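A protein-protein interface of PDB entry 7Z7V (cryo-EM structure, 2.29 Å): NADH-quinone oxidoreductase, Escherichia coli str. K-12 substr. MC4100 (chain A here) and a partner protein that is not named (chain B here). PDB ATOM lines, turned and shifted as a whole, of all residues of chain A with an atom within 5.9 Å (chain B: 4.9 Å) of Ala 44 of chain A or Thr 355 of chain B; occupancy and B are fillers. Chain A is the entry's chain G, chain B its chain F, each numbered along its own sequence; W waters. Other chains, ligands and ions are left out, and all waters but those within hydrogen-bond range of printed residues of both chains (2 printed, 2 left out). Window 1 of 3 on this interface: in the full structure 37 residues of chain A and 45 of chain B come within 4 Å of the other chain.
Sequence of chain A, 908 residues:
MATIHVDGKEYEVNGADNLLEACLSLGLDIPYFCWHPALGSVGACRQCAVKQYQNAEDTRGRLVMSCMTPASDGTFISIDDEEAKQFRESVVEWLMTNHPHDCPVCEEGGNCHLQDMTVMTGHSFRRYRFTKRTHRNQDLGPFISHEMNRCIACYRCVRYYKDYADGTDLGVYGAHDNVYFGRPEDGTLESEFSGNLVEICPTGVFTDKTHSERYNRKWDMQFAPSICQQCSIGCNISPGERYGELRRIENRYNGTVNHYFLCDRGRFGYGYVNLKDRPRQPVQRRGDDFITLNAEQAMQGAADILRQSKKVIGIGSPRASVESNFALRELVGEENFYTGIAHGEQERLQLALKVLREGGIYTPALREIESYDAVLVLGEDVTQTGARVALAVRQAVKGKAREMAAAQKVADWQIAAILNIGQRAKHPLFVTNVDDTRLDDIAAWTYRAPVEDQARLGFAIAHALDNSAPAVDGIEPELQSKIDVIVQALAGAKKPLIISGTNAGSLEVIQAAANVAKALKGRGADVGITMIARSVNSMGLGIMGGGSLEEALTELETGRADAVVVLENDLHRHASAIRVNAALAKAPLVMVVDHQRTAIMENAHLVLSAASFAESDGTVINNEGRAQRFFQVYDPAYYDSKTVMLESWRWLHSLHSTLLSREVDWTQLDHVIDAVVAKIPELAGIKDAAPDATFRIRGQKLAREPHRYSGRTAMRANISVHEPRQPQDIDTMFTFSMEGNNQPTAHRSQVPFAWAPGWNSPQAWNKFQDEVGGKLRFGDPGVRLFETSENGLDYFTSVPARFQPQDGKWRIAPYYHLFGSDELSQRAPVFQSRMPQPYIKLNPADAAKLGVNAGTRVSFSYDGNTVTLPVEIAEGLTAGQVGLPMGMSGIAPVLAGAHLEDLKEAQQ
Among the printed residues, merely in contact across the chains: Val 42 of chain A with Trp 353 of chain B (3.6 Å), Gly 43 of chain A with Trp 353 of chain B (3.9 Å), Ala 44 of chain A with Trp 353 of chain B (3.6 Å), Ala 44 of chain A with Cys 354 of chain B (3.2 Å), Ala 44 of chain A with Thr 355 of chain B (3.6 Å), Arg 46 of chain A with Cys 354 of chain B (3.9 Å), Arg 46 of chain A with Pro 356 of chain B (3.5 Å), Trp 94 of chain A with Thr 355 of chain B (3.97 Å), Trp 94 of chain A with Pro 356 of chain B (3.5 Å), Trp 94 of chain A with Asp 359 of chain B (3.6 Å), Trp 94 of chain A with Gly 360 of chain B (3.98 Å), Leu 95 of chain A with Thr 355 of chain B (3.7 Å), Leu 95 of chain A with Arg 358 of chain B (3.8 Å), Leu 95 of chain A with Asp 359 of chain B (3.9 Å), Ala 153 of chain A with Arg 358 of chain B (3.5 Å) and Tyr 155 of chain A with Trp 353 of chain B (3.4 Å).
SG of Cys 34 of chain A lies close to N of Ala 44 of chain A, at 3.1 Å.
The guanidinium group (NH2) of Arg 358 of chain B is in hydrogen-bond range of the side-chain hydroxyl (OG1) of Thr 355 of chain B (3.1 Å).
The backbone carbonyl oxygen of Trp 353 of chain B is in hydrogen-bond range of the guanidinium group of Arg 358 of chain B, at 3.4 Å.
The backbone carbonyl oxygen (O) of Gly 43 of chain A lies within hydrogen-bond range of the guanidinium group (NH1) of Arg 46 of chain A.
SG of Cys 45 of chain A sits close to N of Gln 47 of chain A (3.4 Å).
NH2 of Arg 358 of chain B is in salt-bridge range of OD2 of Asp 359 of chain B (3.3 Å).
Cys 34 of chain A touches none of the printed residues of chain B.
Of chain B, only Trp 353, Cys 354 and Thr 355 come within 4 Å of Ala 44 of chain A.
Printed residues of chain B within 4 Å of Arg 46 of chain A: Cys 354 (3.9 Å) and Pro 356 (3.5 Å).
Printed residues of chain B within 4 Å of Leu 95 of chain A: Thr 355, Arg 358 and Asp 359.
Cys 154 of chain A touches none of the printed residues of chain B.
Of chain A, only Ala 44, Cys 45, Trp 94 and Leu 95 come within 4 Å of Thr 355 of chain B.
The nearest printed residue of chain B that does not touch Ala 44 of chain A is Pro 356 of chain B (5.2 Å).
The nearest residue of chain A that does not touch Thr 355 of chain B is Val 91 of chain A (4.03 Å).
The nearest printed residue of chain B that does not touch Ile 152 of chain A is Thr 355 of chain B (4.7 Å).
The side-chain hydroxyl (OG1) of Thr 355 of chain B sits at hydrogen-bond distance from the backbone carbonyl oxygen (O) of Cys 45 of chain A, 3.0 Å away.
O of Ile 152 of chain A lies within hydrogen-bond range of NH2 of Arg 358 of chain B (3.1 Å).
Of the 8 printed residues of chain B, 7 touch a printed residue of chain A.
Hydrophobic or aromatic side chains of chain B that line the printed part of chain A: Trp 353 and Pro 356.
Of the 15 printed residues of chain A, 10 touch a printed residue of chain B.
Hydrophobic or aromatic side chains of chain A within 4 Å of the printed part of chain B: Val 42, Ala 44, Trp 94, Leu 95, Ala 153 and Tyr 155.
Along chain A the printed residues that touch a printed residue of chain B span positions 42 to 155.
Among the printed residues, 18 pairs touch across the chains.
Among the printed residues, no Asp or Glu carboxylate lies within 4 Å of a Lys or Arg side-chain nitrogen of the other chain.
Water W2 lies within hydrogen-bond range of O of Ile 152 of chain A, OG1 of Thr 355 of chain B and O of Ala 153 of chain A.
Water W1 lies within hydrogen-bond range of the side-chain carboxylate of Asp 359 of chain B (2.9 Å), the backbone carbonyl oxygen of Ile 152 of chain A (3.4 Å) and the guanidinium group of Arg 358 of chain B (3.5 Å).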
ATOM      1  N   CYS A  34       2.508  20.523  -8.890  1.00  0.00           N
ATOM      2  CA  CYS A  34       1.397  21.369  -8.472  1.00  0.00           C
ATOM      3  C   CYS A  34       0.299  20.601  -7.752  1.00  0.00           C
ATOM      4  O   CYS A  34      -0.501  21.216  -7.045  1.00  0.00           O
ATOM      5  CB  CYS A  34       0.821  22.118  -9.677  1.00  0.00           C
ATOM      6  SG  CYS A  34      -0.135  21.135 -10.826  1.00  0.00           S
ATOM      7  N   VAL A  42      -4.931  20.806 -10.222  1.00  0.00           N
ATOM      8  CA  VAL A  42      -5.191  22.032 -10.969  1.00  0.00           C
ATOM      9  C   VAL A  42      -4.512  21.991 -12.330  1.00  0.00           C
ATOM     10  O   VAL A  42      -4.841  22.780 -13.218  1.00  0.00           O
ATOM     11  CB  VAL A  42      -4.744  23.275 -10.182  1.00  0.00           C
ATOM     12  CG1 VAL A  42      -5.761  23.604  -9.114  1.00  0.00           C
ATOM     13  CG2 VAL A  42      -3.355  23.073  -9.594  1.00  0.00           C
ATOM     14  N   GLY A  43      -3.565  21.076 -12.504  1.00  0.00           N
ATOM     15  CA  GLY A  43      -2.888  20.923 -13.779  1.00  0.00           C
ATOM     16  C   GLY A  43      -2.005  22.080 -14.197  1.00  0.00           C
ATOM     17  O   GLY A  43      -1.976  22.430 -15.380  1.00  0.00           O
ATOM     18  N   ALA A  44      -1.269  22.671 -13.260  1.00  0.00           N
ATOM     19  CA  ALA A  44      -0.453  23.845 -13.551  1.00  0.00           C
ATOM     20  C   ALA A  44       0.945  23.474 -14.042  1.00  0.00           C
ATOM     21  O   ALA A  44       1.340  23.868 -15.137  1.00  0.00           O
ATOM     22  CB  ALA A  44      -0.356  24.742 -12.314  1.00  0.00           C
ATOM     23  N   CYS A  45       1.699  22.710 -13.250  1.00  0.00           N
ATOM     24  CA  CYS A  45       3.123  22.532 -13.518  1.00  0.00           C
ATOM     25  C   CYS A  45       3.408  21.721 -14.777  1.00  0.00           C
ATOM     26  O   CYS A  45       4.521  21.802 -15.301  1.00  0.00           O
ATOM     27  CB  CYS A  45       3.798  21.864 -12.326  1.00  0.00           C
ATOM     28  SG  CYS A  45       3.303  20.166 -12.081  1.00  0.00           S
ATOM     29  N   ARG A  46       2.439  20.941 -15.253  1.00  0.00           N
ATOM     30  CA  ARG A  46       2.540  20.063 -16.423  1.00  0.00           C
ATOM     31  C   ARG A  46       3.629  19.002 -16.280  1.00  0.00           C
ATOM     32  O   ARG A  46       4.103  18.461 -17.278  1.00  0.00           O
ATOM     33  CB  ARG A  46       2.730  20.857 -17.723  1.00  0.00           C
ATOM     34  CG  ARG A  46       1.784  22.035 -17.880  1.00  0.00           C
ATOM     35  CD  ARG A  46       0.343  21.645 -17.716  1.00  0.00           C
ATOM     36  NE  ARG A  46      -0.214  21.030 -18.910  1.00  0.00           N
ATOM     37  CZ  ARG A  46      -1.494  20.734 -19.054  1.00  0.00           C
ATOM     38  NH1 ARG A  46      -2.374  21.005 -18.107  1.00  0.00           N
ATOM     39  NH2 ARG A  46      -1.900  20.138 -20.167  1.00  0.00           N
ATOM     40  N   GLN A  47       4.010  18.662 -15.050  1.00  0.00           N
ATOM     41  CA  GLN A  47       5.077  17.694 -14.831  1.00  0.00           C
ATOM     42  C   GLN A  47       4.596  16.254 -14.960  1.00  0.00           C
ATOM     43  O   GLN A  47       5.363  15.389 -15.387  1.00  0.00           O
ATOM     44  CB  GLN A  47       5.696  17.916 -13.450  1.00  0.00           C
ATOM     45  CG  GLN A  47       6.888  17.051 -13.128  1.00  0.00           C
ATOM     46  CD  GLN A  47       8.032  17.260 -14.084  1.00  0.00           C
ATOM     47  OE1 GLN A  47       8.741  18.253 -14.000  1.00  0.00           O
ATOM     48  NE2 GLN A  47       8.212  16.331 -15.006  1.00  0.00           N
ATOM     49  N   CYS A  67      -2.748  13.879 -13.174  1.00  0.00           N
ATOM     50  CA  CYS A  67      -3.519  14.475 -12.089  1.00  0.00           C
ATOM     51  C   CYS A  67      -4.866  15.005 -12.558  1.00  0.00           C
ATOM     52  O   CYS A  67      -5.790  15.099 -11.750  1.00  0.00           O
ATOM     53  CB  CYS A  67      -2.714  15.592 -11.417  1.00  0.00           C
ATOM     54  SG  CYS A  67      -2.573  17.121 -12.349  1.00  0.00           S
ATOM     55  N   VAL A  91      10.027  19.546 -18.962  1.00  0.00           N
ATOM     56  CA  VAL A  91       9.390  20.383 -17.948  1.00  0.00           C
ATOM     57  C   VAL A  91      10.369  20.696 -16.820  1.00  0.00           C
ATOM     58  O   VAL A  91      10.479  21.850 -16.373  1.00  0.00           O
ATOM     59  CB  VAL A  91       8.105  19.709 -17.429  1.00  0.00           C
ATOM     60  CG1 VAL A  91       7.580  20.417 -16.195  1.00  0.00           C
ATOM     61  CG2 VAL A  91       7.042  19.699 -18.511  1.00  0.00           C
ATOM     62  N   TRP A  94      12.821  23.265 -18.202  1.00  0.00           N
ATOM     63  CA  TRP A  94      12.251  24.609 -18.235  1.00  0.00           C
ATOM     64  C   TRP A  94      12.232  25.231 -16.849  1.00  0.00           C
ATOM     65  O   TRP A  94      12.482  26.432 -16.698  1.00  0.00           O
ATOM     66  CB  TRP A  94      10.838  24.573 -18.812  1.00  0.00           C
ATOM     67  CG  TRP A  94      10.787  24.298 -20.268  1.00  0.00           C
ATOM     68  CD1 TRP A  94      11.655  24.742 -21.216  1.00  0.00           C
ATOM     69  CD2 TRP A  94       9.817  23.504 -20.953  1.00  0.00           C
ATOM     70  NE1 TRP A  94      11.285  24.277 -22.449  1.00  0.00           N
ATOM     71  CE2 TRP A  94      10.159  23.512 -22.315  1.00  0.00           C
ATOM     72  CE3 TRP A  94       8.692  22.786 -20.544  1.00  0.00           C
ATOM     73  CZ2 TRP A  94       9.416  22.830 -23.272  1.00  0.00           C
ATOM     74  CZ3 TRP A  94       7.961  22.107 -21.492  1.00  0.00           C
ATOM     75  CH2 TRP A  94       8.322  22.137 -22.841  1.00  0.00           C
ATOM     76  N   LEU A  95      11.929  24.431 -15.824  1.00  0.00           N
ATOM     77  CA  LEU A  95      12.028  24.935 -14.458  1.00  0.00           C
ATOM     78  C   LEU A  95      13.468  25.267 -14.083  1.00  0.00           C
ATOM     79  O   LEU A  95      13.705  26.199 -13.311  1.00  0.00           O
ATOM     80  CB  LEU A  95      11.447  23.918 -13.481  1.00  0.00           C
ATOM     81  CG  LEU A  95       9.943  23.685 -13.578  1.00  0.00           C
ATOM     82  CD1 LEU A  95       9.512  22.699 -12.525  1.00  0.00           C
ATOM     83  CD2 LEU A  95       9.180  24.987 -13.438  1.00  0.00           C
ATOM     84  N   ILE A 152       9.245  27.784  -8.524  1.00  0.00           N
ATOM     85  CA  ILE A 152       8.957  27.136  -9.793  1.00  0.00           C
ATOM     86  C   ILE A 152       7.538  27.421 -10.259  1.00  0.00           C
ATOM     87  O   ILE A 152       7.085  26.817 -11.234  1.00  0.00           O
ATOM     88  CB  ILE A 152       9.215  25.624  -9.724  1.00  0.00           C
ATOM     89  CG1 ILE A 152       8.325  24.980  -8.660  1.00  0.00           C
ATOM     90  CG2 ILE A 152      10.687  25.347  -9.476  1.00  0.00           C
ATOM     91  CD1 ILE A 152       8.501  23.506  -8.528  1.00  0.00           C
ATOM     92  N   ALA A 153       6.834  28.333  -9.582  1.00  0.00           N
ATOM     93  CA  ALA A 153       5.477  28.768  -9.931  1.00  0.00           C
ATOM     94  C   ALA A 153       4.518  27.585 -10.032  1.00  0.00           C
ATOM     95  O   ALA A 153       3.813  27.399 -11.022  1.00  0.00           O
ATOM     96  CB  ALA A 153       5.472  29.597 -11.217  1.00  0.00           C
ATOM     97  N   CYS A 154       4.528  26.757  -8.998  1.00  0.00           N
ATOM     98  CA  CYS A 154       3.656  25.598  -8.934  1.00  0.00           C
ATOM     99  C   CYS A 154       2.319  25.895  -8.272  1.00  0.00           C
ATOM    100  O   CYS A 154       1.435  25.035  -8.296  1.00  0.00           O
ATOM    101  CB  CYS A 154       4.370  24.467  -8.197  1.00  0.00           C
ATOM    102  SG  CYS A 154       4.325  24.594  -6.416  1.00  0.00           S
ATOM    103  N   TYR A 155       2.164  27.078  -7.676  1.00  0.00           N
ATOM    104  CA  TYR A 155       0.943  27.606  -7.069  1.00  0.00           C
ATOM    105  C   TYR A 155       0.466  26.815  -5.858  1.00  0.00           C
ATOM    106  O   TYR A 155      -0.656  27.027  -5.411  1.00  0.00           O
ATOM    107  CB  TYR A 155      -0.203  27.719  -8.087  1.00  0.00           C
ATOM    108  CG  TYR A 155       0.068  28.704  -9.200  1.00  0.00           C
ATOM    109  CD1 TYR A 155       0.811  28.336 -10.312  1.00  0.00           C
ATOM    110  CD2 TYR A 155      -0.419  30.001  -9.139  1.00  0.00           C
ATOM    111  CE1 TYR A 155       1.071  29.231 -11.322  1.00  0.00           C
ATOM    112  CE2 TYR A 155      -0.168  30.902 -10.148  1.00  0.00           C
ATOM    113  CZ  TYR A 155       0.579  30.512 -11.237  1.00  0.00           C
ATOM    114  OH  TYR A 155       0.835  31.402 -12.247  1.00  0.00           O
ATOM    115  N   TRP B 353       0.490  30.614 -15.759  1.00  0.00           N
ATOM    116  CA  TRP B 353      -0.076  29.504 -15.002  1.00  0.00           C
ATOM    117  C   TRP B 353       0.727  28.226 -15.185  1.00  0.00           C
ATOM    118  O   TRP B 353       0.999  27.518 -14.212  1.00  0.00           O
ATOM    119  CB  TRP B 353      -1.529  29.279 -15.417  1.00  0.00           C
ATOM    120  CG  TRP B 353      -2.193  28.075 -14.844  1.00  0.00           C
ATOM    121  CD1 TRP B 353      -2.575  26.959 -15.518  1.00  0.00           C
ATOM    122  CD2 TRP B 353      -2.592  27.879 -13.486  1.00  0.00           C
ATOM    123  NE1 TRP B 353      -3.176  26.072 -14.666  1.00  0.00           N
ATOM    124  CE2 TRP B 353      -3.198  26.614 -13.409  1.00  0.00           C
ATOM    125  CE3 TRP B 353      -2.485  28.646 -12.324  1.00  0.00           C
ATOM    126  CZ2 TRP B 353      -3.699  26.098 -12.218  1.00  0.00           C
ATOM    127  CZ3 TRP B 353      -2.980  28.133 -11.145  1.00  0.00           C
ATOM    128  CH2 TRP B 353      -3.579  26.872 -11.100  1.00  0.00           C
ATOM    129  N   CYS B 354       1.112  27.906 -16.416  1.00  0.00           N
ATOM    130  CA  CYS B 354       1.661  26.592 -16.702  1.00  0.00           C
ATOM    131  C   CYS B 354       3.066  26.685 -17.279  1.00  0.00           C
ATOM    132  O   CYS B 354       3.386  27.608 -18.031  1.00  0.00           O
ATOM    133  CB  CYS B 354       0.714  25.789 -17.614  1.00  0.00           C
ATOM    134  SG  CYS B 354       0.728  26.096 -19.360  1.00  0.00           S
ATOM    135  N   THR B 355       3.890  25.709 -16.894  1.00  0.00           N
ATOM    136  CA  THR B 355       5.334  25.746 -17.134  1.00  0.00           C
ATOM    137  C   THR B 355       5.757  25.849 -18.599  1.00  0.00           C
ATOM    138  O   THR B 355       6.627  26.687 -18.885  1.00  0.00           O
ATOM    139  CB  THR B 355       5.985  24.526 -16.472  1.00  0.00           C
ATOM    140  OG1 THR B 355       5.699  24.528 -15.072  1.00  0.00           O
ATOM    141  CG2 THR B 355       7.487  24.532 -16.676  1.00  0.00           C
ATOM    142  N   PRO B 356       5.246  25.041 -19.556  1.00  0.00           N
ATOM    143  CA  PRO B 356       5.821  25.090 -20.914  1.00  0.00           C
ATOM    144  C   PRO B 356       5.712  26.442 -21.581  1.00  0.00           C
ATOM    145  O   PRO B 356       6.714  26.938 -22.088  1.00  0.00           O
ATOM    146  CB  PRO B 356       5.016  24.027 -21.673  1.00  0.00           C
ATOM    147  CG  PRO B 356       4.520  23.138 -20.640  1.00  0.00           C
ATOM    148  CD  PRO B 356       4.161  24.047 -19.532  1.00  0.00           C
ATOM    149  N   CYS B 357       4.559  27.095 -21.504  1.00  0.00           N
ATOM    150  CA  CYS B 357       4.434  28.421 -22.094  1.00  0.00           C
ATOM    151  C   CYS B 357       5.260  29.444 -21.321  1.00  0.00           C
ATOM    152  O   CYS B 357       6.162  30.069 -21.892  1.00  0.00           O
ATOM    153  CB  CYS B 357       2.957  28.796 -22.151  1.00  0.00           C
ATOM    154  SG  CYS B 357       2.456  30.510 -22.217  1.00  0.00           S
ATOM    155  N   ARG B 358       5.071  29.492 -19.996  1.00  0.00           N
ATOM    156  CA  ARG B 358       5.660  30.531 -19.149  1.00  0.00           C
ATOM    157  C   ARG B 358       7.184  30.486 -19.151  1.00  0.00           C
ATOM    158  O   ARG B 358       7.841  31.530 -19.112  1.00  0.00           O
ATOM    159  CB  ARG B 358       5.119  30.393 -17.722  1.00  0.00           C
ATOM    160  CG  ARG B 358       5.813  31.251 -16.675  1.00  0.00           C
ATOM    161  CD  ARG B 358       5.452  30.843 -15.258  1.00  0.00           C
ATOM    162  NE  ARG B 358       6.177  29.656 -14.827  1.00  0.00           N
ATOM    163  CZ  ARG B 358       5.604  28.498 -14.537  1.00  0.00           C
ATOM    164  NH1 ARG B 358       4.291  28.346 -14.590  1.00  0.00           N
ATOM    165  NH2 ARG B 358       6.367  27.469 -14.186  1.00  0.00           N
ATOM    166  N   ASP B 359       7.766  29.292 -19.213  1.00  0.00           N
ATOM    167  CA  ASP B 359       9.208  29.138 -19.142  1.00  0.00           C
ATOM    168  C   ASP B 359       9.838  28.596 -20.416  1.00  0.00           C
ATOM    169  O   ASP B 359      11.053  28.386 -20.437  1.00  0.00           O
ATOM    170  CB  ASP B 359       9.582  28.227 -17.966  1.00  0.00           C
ATOM    171  CG  ASP B 359       9.447  28.923 -16.627  1.00  0.00           C
ATOM    172  OD1 ASP B 359       9.510  30.166 -16.590  1.00  0.00           O
ATOM    173  OD2 ASP B 359       9.273  28.227 -15.608  1.00  0.00           O
ATOM    174  N   GLY B 360       9.074  28.390 -21.485  1.00  0.00           N
ATOM    175  CA  GLY B 360       9.662  27.907 -22.708  1.00  0.00           C
ATOM    176  C   GLY B 360       9.523  28.914 -23.822  1.00  0.00           C
ATOM    177  O   GLY B 360      10.368  28.951 -24.717  1.00  0.00           O
HETATM  178  O   HOH W   1       9.170  29.009 -12.828  1.00  0.00           O
HETATM  179  O   HOH W   2       5.696  24.577 -11.735  1.00  0.00           O
